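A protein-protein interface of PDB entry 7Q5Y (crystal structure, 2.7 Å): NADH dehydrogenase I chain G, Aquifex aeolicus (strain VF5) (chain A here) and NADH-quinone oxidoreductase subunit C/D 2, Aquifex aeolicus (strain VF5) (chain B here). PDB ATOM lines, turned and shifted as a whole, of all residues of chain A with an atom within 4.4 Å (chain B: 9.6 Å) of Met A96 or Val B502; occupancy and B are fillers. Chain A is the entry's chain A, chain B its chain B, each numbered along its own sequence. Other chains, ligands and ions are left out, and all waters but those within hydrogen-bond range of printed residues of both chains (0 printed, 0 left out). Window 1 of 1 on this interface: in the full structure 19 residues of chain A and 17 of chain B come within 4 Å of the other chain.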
ATOM      1  N   LEU A  92       3.348   1.455 -16.064  1.00  0.00           N
ATOM      2  CA  LEU A  92       3.848   1.081 -17.382  1.00  0.00           C
ATOM      3  C   LEU A  92       2.773   0.362 -18.187  1.00  0.00           C
ATOM      4  O   LEU A  92       2.651   0.581 -19.397  1.00  0.00           O
ATOM      5  CB  LEU A  92       5.123   0.256 -17.260  1.00  0.00           C
ATOM      6  CG  LEU A  92       6.242   1.181 -16.752  1.00  0.00           C
ATOM      7  CD1 LEU A  92       7.434   0.453 -16.153  1.00  0.00           C
ATOM      8  CD2 LEU A  92       6.688   2.076 -17.848  1.00  0.00           C
ATOM      9  N   GLN A  93       1.960  -0.476 -17.538  1.00  0.00           N
ATOM     10  CA  GLN A  93       0.888  -1.137 -18.280  1.00  0.00           C
ATOM     11  C   GLN A  93      -0.126  -0.118 -18.790  1.00  0.00           C
ATOM     12  O   GLN A  93      -0.666  -0.255 -19.901  1.00  0.00           O
ATOM     13  CB  GLN A  93       0.181  -2.169 -17.409  1.00  0.00           C
ATOM     14  CG  GLN A  93      -1.149  -2.624 -17.993  1.00  0.00           C
ATOM     15  CD  GLN A  93      -0.989  -3.479 -19.227  1.00  0.00           C
ATOM     16  OE1 GLN A  93      -1.107  -4.695 -19.162  1.00  0.00           O
ATOM     17  NE2 GLN A  93      -0.724  -2.852 -20.352  1.00  0.00           N
ATOM     18  N   ALA A  94      -0.403   0.905 -17.977  1.00  0.00           N
ATOM     19  CA  ALA A  94      -1.342   1.941 -18.380  1.00  0.00           C
ATOM     20  C   ALA A  94      -0.826   2.665 -19.606  1.00  0.00           C
ATOM     21  O   ALA A  94      -1.577   2.928 -20.558  1.00  0.00           O
ATOM     22  CB  ALA A  94      -1.597   2.915 -17.225  1.00  0.00           C
ATOM     23  N   LEU A  95       0.458   3.011 -19.602  1.00  0.00           N
ATOM     24  CA  LEU A  95       0.987   3.686 -20.776  1.00  0.00           C
ATOM     25  C   LEU A  95       0.861   2.798 -22.010  1.00  0.00           C
ATOM     26  O   LEU A  95       0.506   3.274 -23.088  1.00  0.00           O
ATOM     27  CB  LEU A  95       2.433   4.135 -20.530  1.00  0.00           C
ATOM     28  CG  LEU A  95       2.561   5.284 -19.507  1.00  0.00           C
ATOM     29  CD1 LEU A  95       3.999   5.672 -19.184  1.00  0.00           C
ATOM     30  CD2 LEU A  95       1.847   6.472 -20.027  1.00  0.00           C
ATOM     31  N   MET A  96       1.105   1.496 -21.869  1.00  0.00           N
ATOM     32  CA  MET A  96       1.052   0.600 -23.025  1.00  0.00           C
ATOM     33  C   MET A  96      -0.342   0.267 -23.518  1.00  0.00           C
ATOM     34  O   MET A  96      -0.467  -0.315 -24.594  1.00  0.00           O
ATOM     35  CB  MET A  96       1.781  -0.699 -22.701  1.00  0.00           C
ATOM     36  CG  MET A  96       3.255  -0.462 -22.474  1.00  0.00           C
ATOM     37  SD  MET A  96       4.102  -1.955 -22.004  1.00  0.00           S
ATOM     38  CE  MET A  96       5.804  -1.438 -21.950  1.00  0.00           C
ATOM     39  N   THR A  97      -1.379   0.605 -22.774  1.00  0.00           N
ATOM     40  CA  THR A  97      -2.734   0.255 -23.178  1.00  0.00           C
ATOM     41  C   THR A  97      -3.060   0.638 -24.615  1.00  0.00           C
ATOM     42  O   THR A  97      -3.534  -0.194 -25.389  1.00  0.00           O
ATOM     43  CB  THR A  97      -3.706   0.880 -22.204  1.00  0.00           C
ATOM     44  OG1 THR A  97      -3.797  -0.002 -21.084  1.00  0.00           O
ATOM     45  CG2 THR A  97      -5.033   1.043 -22.852  1.00  0.00           C
ATOM     46  N   ARG A  98      -2.838   1.890 -24.998  1.00  0.00           N
ATOM     47  CA  ARG A  98      -3.133   2.269 -26.376  1.00  0.00           C
ATOM     48  C   ARG A  98      -1.866   2.575 -27.158  1.00  0.00           C
ATOM     49  O   ARG A  98      -1.933   3.179 -28.229  1.00  0.00           O
ATOM     50  CB  ARG A  98      -4.107   3.445 -26.457  1.00  0.00           C
ATOM     51  CG  ARG A  98      -5.446   3.167 -25.830  1.00  0.00           C
ATOM     52  CD  ARG A  98      -6.230   2.065 -26.498  1.00  0.00           C
ATOM     53  NE  ARG A  98      -7.301   1.658 -25.595  1.00  0.00           N
ATOM     54  CZ  ARG A  98      -8.339   0.896 -25.923  1.00  0.00           C
ATOM     55  NH1 ARG A  98      -8.483   0.437 -27.153  1.00  0.00           N
ATOM     56  NH2 ARG A  98      -9.248   0.602 -25.006  1.00  0.00           N
ATOM     57  N   HIS A  99      -0.713   2.180 -26.639  1.00  0.00           N
ATOM     58  CA  HIS A  99       0.535   2.399 -27.345  1.00  0.00           C
ATOM     59  C   HIS A  99       0.637   1.366 -28.464  1.00  0.00           C
ATOM     60  O   HIS A  99       0.479   0.167 -28.206  1.00  0.00           O
ATOM     61  CB  HIS A  99       1.703   2.268 -26.404  1.00  0.00           C
ATOM     62  CG  HIS A  99       2.905   3.024 -26.847  1.00  0.00           C
ATOM     63  ND1 HIS A  99       3.253   4.218 -26.262  1.00  0.00           N
ATOM     64  CD2 HIS A  99       3.810   2.808 -27.832  1.00  0.00           C
ATOM     65  CE1 HIS A  99       4.337   4.695 -26.843  1.00  0.00           C
ATOM     66  NE2 HIS A  99       4.686   3.873 -27.809  1.00  0.00           N
ATOM     67  N   LEU A 114       9.981   4.267 -22.772  1.00  0.00           N
ATOM     68  CA  LEU A 114       8.899   3.309 -22.539  1.00  0.00           C
ATOM     69  C   LEU A 114       9.344   1.896 -22.862  1.00  0.00           C
ATOM     70  O   LEU A 114       9.046   0.956 -22.124  1.00  0.00           O
ATOM     71  CB  LEU A 114       7.670   3.664 -23.374  1.00  0.00           C
ATOM     72  CG  LEU A 114       6.536   2.644 -23.338  1.00  0.00           C
ATOM     73  CD1 LEU A 114       6.078   2.537 -21.972  1.00  0.00           C
ATOM     74  CD2 LEU A 114       5.400   3.156 -24.175  1.00  0.00           C
ATOM     75  N   GLN A 115      10.061   1.731 -23.956  1.00  0.00           N
ATOM     76  CA  GLN A 115      10.533   0.411 -24.319  1.00  0.00           C
ATOM     77  C   GLN A 115      11.528  -0.101 -23.289  1.00  0.00           C
ATOM     78  O   GLN A 115      11.466  -1.265 -22.889  1.00  0.00           O
ATOM     79  CB  GLN A 115      11.140   0.465 -25.719  1.00  0.00           C
ATOM     80  CG  GLN A 115      11.481  -0.870 -26.301  1.00  0.00           C
ATOM     81  CD  GLN A 115      12.237  -0.723 -27.576  1.00  0.00           C
ATOM     82  OE1 GLN A 115      13.456  -0.450 -27.584  1.00  0.00           O
ATOM     83  NE2 GLN A 115      11.515  -0.829 -28.682  1.00  0.00           N
ATOM     84  N   GLY A 118       9.626  -0.281 -19.826  1.00  0.00           N
ATOM     85  CA  GLY A 118       8.574  -1.274 -19.919  1.00  0.00           C
ATOM     86  C   GLY A 118       9.102  -2.684 -19.888  1.00  0.00           C
ATOM     87  O   GLY A 118       8.413  -3.606 -19.438  1.00  0.00           O
ATOM     88  N   ALA A 119      10.316  -2.877 -20.366  1.00  0.00           N
ATOM     89  CA  ALA A 119      10.897  -4.203 -20.384  1.00  0.00           C
ATOM     90  C   ALA A 119      11.564  -4.571 -19.075  1.00  0.00           C
ATOM     91  O   ALA A 119      11.687  -5.758 -18.765  1.00  0.00           O
ATOM     92  CB  ALA A 119      11.923  -4.268 -21.512  1.00  0.00           C
ATOM     93  N   LYS A 135      -5.198   0.444 -31.206  1.00  0.00           N
ATOM     94  CA  LYS A 135      -4.298   1.326 -30.458  1.00  0.00           C
ATOM     95  C   LYS A 135      -4.420   2.765 -30.960  1.00  0.00           C
ATOM     96  O   LYS A 135      -3.534   3.317 -31.624  1.00  0.00           O
ATOM     97  CB  LYS A 135      -2.871   0.817 -30.578  1.00  0.00           C
ATOM     98  CG  LYS A 135      -2.410   0.106 -29.360  1.00  0.00           C
ATOM     99  CD  LYS A 135      -2.795  -1.329 -29.321  1.00  0.00           C
ATOM    100  CE  LYS A 135      -2.698  -1.830 -27.870  1.00  0.00           C
ATOM    101  NZ  LYS A 135      -1.360  -1.758 -27.203  1.00  0.00           N
ATOM    102  N   PRO B 485      12.478 -10.363 -16.781  1.00  0.00           N
ATOM    103  CA  PRO B 485      12.851  -9.440 -17.870  1.00  0.00           C
ATOM    104  C   PRO B 485      13.966  -9.923 -18.779  1.00  0.00           C
ATOM    105  O   PRO B 485      14.087  -9.407 -19.893  1.00  0.00           O
ATOM    106  CB  PRO B 485      13.285  -8.172 -17.120  1.00  0.00           C
ATOM    107  CG  PRO B 485      12.682  -8.291 -15.783  1.00  0.00           C
ATOM    108  CD  PRO B 485      12.667  -9.759 -15.461  1.00  0.00           C
ATOM    109  N   ALA B 486      14.783 -10.878 -18.361  1.00  0.00           N
ATOM    110  CA  ALA B 486      15.878 -11.328 -19.201  1.00  0.00           C
ATOM    111  C   ALA B 486      15.493 -12.486 -20.116  1.00  0.00           C
ATOM    112  O   ALA B 486      16.363 -13.041 -20.788  1.00  0.00           O
ATOM    113  CB  ALA B 486      17.075 -11.725 -18.324  1.00  0.00           C
ATOM    114  N   VAL B 487      14.222 -12.865 -20.158  1.00  0.00           N
ATOM    115  CA  VAL B 487      13.768 -13.990 -20.964  1.00  0.00           C
ATOM    116  C   VAL B 487      13.041 -13.476 -22.203  1.00  0.00           C
ATOM    117  O   VAL B 487      11.957 -12.887 -22.097  1.00  0.00           O
ATOM    118  CB  VAL B 487      12.870 -14.917 -20.135  1.00  0.00           C
ATOM    119  CG1 VAL B 487      12.341 -16.057 -20.994  1.00  0.00           C
ATOM    120  CG2 VAL B 487      13.636 -15.445 -18.926  1.00  0.00           C
ATOM    121  N   ILE B 488      13.622 -13.725 -23.376  1.00  0.00           N
ATOM    122  CA  ILE B 488      13.029 -13.321 -24.649  1.00  0.00           C
ATOM    123  C   ILE B 488      11.749 -14.118 -24.880  1.00  0.00           C
ATOM    124  O   ILE B 488      11.779 -15.361 -24.913  1.00  0.00           O
ATOM    125  CB  ILE B 488      14.010 -13.497 -25.822  1.00  0.00           C
ATOM    126  CG1 ILE B 488      15.225 -12.600 -25.657  1.00  0.00           C
ATOM    127  CG2 ILE B 488      13.342 -13.271 -27.171  1.00  0.00           C
ATOM    128  CD1 ILE B 488      16.403 -13.083 -26.438  1.00  0.00           C
ATOM    129  N   PRO B 489      10.616 -13.447 -25.054  1.00  0.00           N
ATOM    130  CA  PRO B 489       9.343 -14.150 -25.274  1.00  0.00           C
ATOM    131  C   PRO B 489       9.249 -14.721 -26.679  1.00  0.00           C
ATOM    132  O   PRO B 489       9.888 -14.210 -27.613  1.00  0.00           O
ATOM    133  CB  PRO B 489       8.293 -13.051 -25.045  1.00  0.00           C
ATOM    134  CG  PRO B 489       9.018 -11.774 -25.381  1.00  0.00           C
ATOM    135  CD  PRO B 489      10.459 -11.984 -24.981  1.00  0.00           C
ATOM    136  N   ASP B 493       4.092 -14.263 -28.952  1.00  0.00           N
ATOM    137  CA  ASP B 493       3.730 -13.229 -27.981  1.00  0.00           C
ATOM    138  C   ASP B 493       3.945 -11.841 -28.559  1.00  0.00           C
ATOM    139  O   ASP B 493       3.100 -10.953 -28.404  1.00  0.00           O
ATOM    140  CB  ASP B 493       4.596 -13.319 -26.719  1.00  0.00           C
ATOM    141  CG  ASP B 493       4.285 -14.513 -25.837  1.00  0.00           C
ATOM    142  OD1 ASP B 493       3.358 -15.293 -26.142  1.00  0.00           O
ATOM    143  OD2 ASP B 493       5.000 -14.650 -24.812  1.00  0.00           O
ATOM    144  N   VAL B 494       5.074 -11.646 -29.242  1.00  0.00           N
ATOM    145  CA  VAL B 494       5.405 -10.352 -29.821  1.00  0.00           C
ATOM    146  C   VAL B 494       4.455  -9.999 -30.969  1.00  0.00           C
ATOM    147  O   VAL B 494       4.156  -8.822 -31.193  1.00  0.00           O
ATOM    148  CB  VAL B 494       6.889 -10.358 -30.238  1.00  0.00           C
ATOM    149  CG1 VAL B 494       7.280  -9.037 -30.856  1.00  0.00           C
ATOM    150  CG2 VAL B 494       7.788 -10.687 -29.031  1.00  0.00           C
ATOM    151  N   PHE B 495       3.955 -10.993 -31.706  1.00  0.00           N
ATOM    152  CA  PHE B 495       3.013 -10.707 -32.784  1.00  0.00           C
ATOM    153  C   PHE B 495       1.692 -10.210 -32.253  1.00  0.00           C
ATOM    154  O   PHE B 495       0.881  -9.697 -33.028  1.00  0.00           O
ATOM    155  CB  PHE B 495       2.631 -11.965 -33.596  1.00  0.00           C
ATOM    156  CG  PHE B 495       3.758 -12.644 -34.313  1.00  0.00           C
ATOM    157  CD1 PHE B 495       4.920 -11.966 -34.645  1.00  0.00           C
ATOM    158  CD2 PHE B 495       3.626 -13.970 -34.689  1.00  0.00           C
ATOM    159  CE1 PHE B 495       5.944 -12.609 -35.326  1.00  0.00           C
ATOM    160  CE2 PHE B 495       4.643 -14.618 -35.367  1.00  0.00           C
ATOM    161  CZ  PHE B 495       5.805 -13.935 -35.691  1.00  0.00           C
ATOM    162  N   HIS B 496       1.455 -10.406 -30.957  1.00  0.00           N
ATOM    163  CA  HIS B 496       0.206 -10.142 -30.260  1.00  0.00           C
ATOM    164  C   HIS B 496       0.119  -8.861 -29.434  1.00  0.00           C
ATOM    165  O   HIS B 496      -0.903  -8.167 -29.512  1.00  0.00           O
ATOM    166  CB  HIS B 496      -0.089 -11.340 -29.348  1.00  0.00           C
ATOM    167  CG  HIS B 496      -1.348 -11.188 -28.557  1.00  0.00           C
ATOM    168  ND1 HIS B 496      -1.359 -10.701 -27.269  1.00  0.00           N
ATOM    169  CD2 HIS B 496      -2.643 -11.387 -28.896  1.00  0.00           C
ATOM    170  CE1 HIS B 496      -2.604 -10.646 -26.834  1.00  0.00           C
ATOM    171  NE2 HIS B 496      -3.402 -11.051 -27.803  1.00  0.00           N
ATOM    172  N   ASP B 497       1.111  -8.561 -28.592  1.00  0.00           N
ATOM    173  CA  ASP B 497       0.992  -7.403 -27.717  1.00  0.00           C
ATOM    174  C   ASP B 497       2.310  -6.668 -27.529  1.00  0.00           C
ATOM    175  O   ASP B 497       3.398  -7.240 -27.628  1.00  0.00           O
ATOM    176  CB  ASP B 497       0.437  -7.826 -26.345  1.00  0.00           C
ATOM    177  CG  ASP B 497       1.179  -9.033 -25.740  1.00  0.00           C
ATOM    178  OD1 ASP B 497       2.297  -8.841 -25.205  1.00  0.00           O
ATOM    179  OD2 ASP B 497       0.669 -10.176 -25.825  1.00  0.00           O
ATOM    180  N   LEU B 498       2.181  -5.369 -27.246  1.00  0.00           N
ATOM    181  CA  LEU B 498       3.349  -4.523 -27.053  1.00  0.00           C
ATOM    182  C   LEU B 498       4.109  -4.889 -25.794  1.00  0.00           C
ATOM    183  O   LEU B 498       5.338  -4.758 -25.754  1.00  0.00           O
ATOM    184  CB  LEU B 498       2.912  -3.064 -27.011  1.00  0.00           C
ATOM    185  CG  LEU B 498       3.947  -2.056 -26.539  1.00  0.00           C
ATOM    186  CD1 LEU B 498       4.954  -1.780 -27.645  1.00  0.00           C
ATOM    187  CD2 LEU B 498       3.238  -0.798 -26.136  1.00  0.00           C
ATOM    188  N   GLU B 499       3.395  -5.353 -24.765  1.00  0.00           N
ATOM    189  CA  GLU B 499       4.016  -5.722 -23.497  1.00  0.00           C
ATOM    190  C   GLU B 499       5.079  -6.803 -23.683  1.00  0.00           C
ATOM    191  O   GLU B 499       6.022  -6.886 -22.889  1.00  0.00           O
ATOM    192  CB  GLU B 499       2.938  -6.153 -22.503  1.00  0.00           C
ATOM    193  CG  GLU B 499       1.937  -5.041 -22.125  1.00  0.00           C
ATOM    194  CD  GLU B 499       0.743  -4.912 -23.079  1.00  0.00           C
ATOM    195  OE1 GLU B 499       0.807  -5.385 -24.246  1.00  0.00           O
ATOM    196  OE2 GLU B 499      -0.279  -4.324 -22.643  1.00  0.00           O
ATOM    197  N   SER B 500       4.945  -7.641 -24.719  1.00  0.00           N
ATOM    198  CA  SER B 500       5.943  -8.668 -24.988  1.00  0.00           C
ATOM    199  C   SER B 500       7.004  -8.149 -25.947  1.00  0.00           C
ATOM    200  O   SER B 500       8.196  -8.425 -25.772  1.00  0.00           O
ATOM    201  CB  SER B 500       5.293  -9.922 -25.580  1.00  0.00           C
ATOM    202  OG  SER B 500       4.508 -10.623 -24.626  1.00  0.00           O
ATOM    203  N   MET B 501       6.576  -7.363 -26.932  1.00  0.00           N
ATOM    204  CA  MET B 501       7.492  -6.808 -27.921  1.00  0.00           C
ATOM    205  C   MET B 501       8.639  -6.021 -27.284  1.00  0.00           C
ATOM    206  O   MET B 501       9.808  -6.203 -27.653  1.00  0.00           O
ATOM    207  CB  MET B 501       6.698  -5.931 -28.889  1.00  0.00           C
ATOM    208  CG  MET B 501       7.504  -5.251 -29.972  1.00  0.00           C
ATOM    209  SD  MET B 501       6.465  -4.981 -31.424  1.00  0.00           S
ATOM    210  CE  MET B 501       6.049  -3.335 -31.147  1.00  0.00           C
ATOM    211  N   VAL B 502       8.333  -5.142 -26.322  1.00  0.00           N
ATOM    212  CA  VAL B 502       9.387  -4.324 -25.717  1.00  0.00           C
ATOM    213  C   VAL B 502      10.447  -5.168 -25.029  1.00  0.00           C
ATOM    214  O   VAL B 502      11.602  -4.741 -24.914  1.00  0.00           O
ATOM    215  CB  VAL B 502       8.777  -3.287 -24.767  1.00  0.00           C
ATOM    216  CG1 VAL B 502       7.711  -2.532 -25.517  1.00  0.00           C
ATOM    217  CG2 VAL B 502       8.213  -3.979 -23.513  1.00  0.00           C
ATOM    218  N   LYS B 503      10.087  -6.368 -24.568  1.00  0.00           N
ATOM    219  CA  LYS B 503      11.075  -7.236 -23.936  1.00  0.00           C
ATOM    220  C   LYS B 503      12.044  -7.771 -24.977  1.00  0.00           C
ATOM    221  O   LYS B 503      13.260  -7.797 -24.753  1.00  0.00           O
ATOM    222  CB  LYS B 503      10.383  -8.382 -23.205  1.00  0.00           C
ATOM    223  CG  LYS B 503       9.437  -7.954 -22.097  1.00  0.00           C
ATOM    224  CD  LYS B 503       8.959  -9.174 -21.348  1.00  0.00           C
ATOM    225  CE  LYS B 503      10.144 -10.002 -20.917  1.00  0.00           C
ATOM    226  NZ  LYS B 503       9.716 -11.168 -20.132  1.00  0.00           N
ATOM    227  N   SER B 504      11.507  -8.206 -26.121  1.00  0.00           N
ATOM    228  CA  SER B 504      12.328  -8.719 -27.209  1.00  0.00           C
ATOM    229  C   SER B 504      13.327  -7.668 -27.665  1.00  0.00           C
ATOM    230  O   SER B 504      14.523  -7.946 -27.825  1.00  0.00           O
ATOM    231  CB  SER B 504      11.422  -9.142 -28.370  1.00  0.00           C
ATOM    232  OG  SER B 504      12.153  -9.561 -29.515  1.00  0.00           O
ATOM    233  N   PHE B 505      12.851  -6.440 -27.859  1.00  0.00           N
ATOM    234  CA  PHE B 505      13.736  -5.380 -28.303  1.00  0.00           C
ATOM    235  C   PHE B 505      14.799  -5.072 -27.263  1.00  0.00           C
ATOM    236  O   PHE B 505      15.975  -4.919 -27.601  1.00  0.00           O
ATOM    237  CB  PHE B 505      12.928  -4.133 -28.654  1.00  0.00           C
ATOM    238  CG  PHE B 505      12.449  -4.111 -30.078  1.00  0.00           C
ATOM    239  CD1 PHE B 505      11.330  -4.846 -30.465  1.00  0.00           C
ATOM    240  CD2 PHE B 505      13.149  -3.391 -31.047  1.00  0.00           C
ATOM    241  CE1 PHE B 505      10.884  -4.833 -31.785  1.00  0.00           C
ATOM    242  CE2 PHE B 505      12.724  -3.387 -32.382  1.00  0.00           C
ATOM    243  CZ  PHE B 505      11.595  -4.108 -32.753  1.00  0.00           C
ATOM    244  N   ARG B 506      14.409  -4.970 -25.996  1.00  0.00           N
ATOM    245  CA  ARG B 506      15.376  -4.643 -24.947  1.00  0.00           C
ATOM    246  C   ARG B 506      16.535  -5.623 -24.919  1.00  0.00           C
ATOM    247  O   ARG B 506      17.706  -5.228 -24.968  1.00  0.00           O
ATOM    248  CB  ARG B 506      14.690  -4.659 -23.587  1.00  0.00           C
ATOM    249  CG  ARG B 506      15.094  -3.572 -22.615  1.00  0.00           C
ATOM    250  CD  ARG B 506      16.502  -3.645 -22.073  1.00  0.00           C
ATOM    251  NE  ARG B 506      17.139  -2.342 -22.271  1.00  0.00           N
ATOM    252  CZ  ARG B 506      18.072  -1.809 -21.489  1.00  0.00           C
ATOM    253  NH1 ARG B 506      18.494  -2.451 -20.413  1.00  0.00           N
ATOM    254  NH2 ARG B 506      18.578  -0.622 -21.791  1.00  0.00           N
ATOM    255  N   VAL B 507      16.218  -6.911 -24.826  1.00  0.00           N
ATOM    256  CA  VAL B 507      17.242  -7.938 -24.698  1.00  0.00           C
ATOM    257  C   VAL B 507      18.073  -8.055 -25.961  1.00  0.00           C
ATOM    258  O   VAL B 507      19.297  -8.217 -25.906  1.00  0.00           O
ATOM    259  CB  VAL B 507      16.576  -9.272 -24.334  1.00  0.00           C
ATOM    260  CG1 VAL B 507      17.620 -10.330 -24.106  1.00  0.00           C
ATOM    261  CG2 VAL B 507      15.709  -9.070 -23.134  1.00  0.00           C
ATOM    262  N   VAL B 508      17.426  -8.025 -27.116  1.00  0.00           N
ATOM    263  CA  VAL B 508      18.168  -8.154 -28.359  1.00  0.00           C
ATOM    264  C   VAL B 508      19.093  -6.955 -28.595  1.00  0.00           C
ATOM    265  O   VAL B 508      20.220  -7.115 -29.082  1.00  0.00           O
ATOM    266  CB  VAL B 508      17.184  -8.364 -29.521  1.00  0.00           C
ATOM    267  CG1 VAL B 508      17.860  -8.090 -30.841  1.00  0.00           C
ATOM    268  CG2 VAL B 508      16.669  -9.767 -29.482  1.00  0.00           C
ATOM    269  N   VAL B 509      18.651  -5.741 -28.261  1.00  0.00           N
ATOM    270  CA  VAL B 509      19.494  -4.588 -28.551  1.00  0.00           C
ATOM    271  C   VAL B 509      20.535  -4.345 -27.472  1.00  0.00           C
ATOM    272  O   VAL B 509      21.691  -4.037 -27.779  1.00  0.00           O
ATOM    273  CB  VAL B 509      18.636  -3.333 -28.792  1.00  0.00           C
ATOM    274  CG1 VAL B 509      19.520  -2.105 -28.921  1.00  0.00           C
ATOM    275  CG2 VAL B 509      17.783  -3.488 -30.027  1.00  0.00           C
ATOM    276  N   HIS B 510      20.160  -4.448 -26.207  1.00  0.00           N
ATOM    277  CA  HIS B 510      21.087  -4.168 -25.117  1.00  0.00           C
ATOM    278  C   HIS B 510      21.615  -5.385 -24.370  1.00  0.00           C
ATOM    279  O   HIS B 510      22.596  -5.250 -23.629  1.00  0.00           O
ATOM    280  CB  HIS B 510      20.404  -3.244 -24.088  1.00  0.00           C
ATOM    281  CG  HIS B 510      19.855  -1.983 -24.678  1.00  0.00           C
ATOM    282  ND1 HIS B 510      20.624  -0.856 -24.879  1.00  0.00           N
ATOM    283  CD2 HIS B 510      18.617  -1.679 -25.140  1.00  0.00           C
ATOM    284  CE1 HIS B 510      19.882   0.085 -25.435  1.00  0.00           C
ATOM    285  NE2 HIS B 510      18.661  -0.389 -25.604  1.00  0.00           N
ATOM    286  N   GLY B 511      21.011  -6.556 -24.537  1.00  0.00           N
ATOM    287  CA  GLY B 511      21.414  -7.726 -23.788  1.00  0.00           C
ATOM    288  C   GLY B 511      20.681  -7.765 -22.449  1.00  0.00           C
ATOM    289  O   GLY B 511      20.012  -6.816 -22.030  1.00  0.00           O
ATOM    290  N   ASP B 513      20.001  -7.602 -18.492  1.00  0.00           N
ATOM    291  CA  ASP B 513      20.534  -6.698 -17.470  1.00  0.00           C
ATOM    292  C   ASP B 513      21.178  -7.513 -16.352  1.00  0.00           C
ATOM    293  O   ASP B 513      20.666  -7.625 -15.238  1.00  0.00           O
ATOM    294  CB  ASP B 513      19.441  -5.792 -16.935  1.00  0.00           C
ATOM    295  CG  ASP B 513      19.043  -4.741 -17.934  1.00  0.00           C
ATOM    296  OD1 ASP B 513      18.429  -5.102 -18.972  1.00  0.00           O
ATOM    297  OD2 ASP B 513      19.368  -3.559 -17.686  1.00  0.00           O
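OE2 of Glu B499 lies within hydrogen-bond range of NE2 of Gln A93 (2.8 Å).
The backbone carbonyl oxygen of Gln A93 is in hydrogen-bond range of the side-chain hydroxyl of Thr A97, at 3.4 Å. The side-chain amino group (NZ) of Lys A135 is in hydrogen-bond range of the backbone carbonyl oxygen (O) of Met A96. O of His A99 sits at hydrogen-bond distance from NZ of Lys A135. The backbone carbonyl oxygen of Val B487 sits at hydrogen-bond distance from the side-chain amino group of Lys B503, at 3.4 Å. NH1 of Arg B506 lies within salt-bridge range of OD1 of Asp B513 (3.0 Å).
Among the printed residues, pairs that only touch across the chains: Ala A119 with Pro B485, Ala A119 with Arg B506, His A99 with Leu B498, Ala A119 with Val B502, Gln A115 with Phe B505, Met A96 with Leu B498, Met A96 with Glu B499, Met A96 with Val B502, Gln A115 with Val B502, Ala A119 with Lys B503 and Gly A118 with Val B502.
Of the printed residues of chain B, Met A96 touches Leu B498, Glu B499 and Val B502. No residue of chain B comes within 4 Å of Thr A97. Gly A118 touches just one residue of chain B: Val B502 (3.95 Å). Of the printed residues of chain A, Leu B498 touches Met A96 (3.7 Å) and His A99 (3.4 Å). Printed residues of chain A within 4 Å of Val B502: Met A96, Gln A115, Gly A118 and Ala A119. Printed residues of chain A within 4 Å of Lys B503: Ala A119 (3.9 Å). Of the printed residues of chain A, Phe B505 touches Gln A115. Val B508 touches none of the printed residues of chain A.
Of the 13 printed residues of chain A, 6 touch a printed residue of chain B. Hydrophobic or aromatic side chains of chain A that line the printed part of chain B: Met A96, His A99 and Ala A119. Printed residues of chain B that touch a printed residue of chain A: Pro B485, Leu B498, Glu B499, Val B502, Lys B503, Phe B505 and Arg B506. Hydrophobic or aromatic side chains of chain B that line the printed part of chain A: Pro B485, Leu B498, Val B502 and Phe B505. Among the printed residues, 12 pairs touch across the chains. Among the printed residues, no Asp or Glu carboxylate lies within 4 Å of a Lys or Arg side-chain nitrogen of the other chain.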
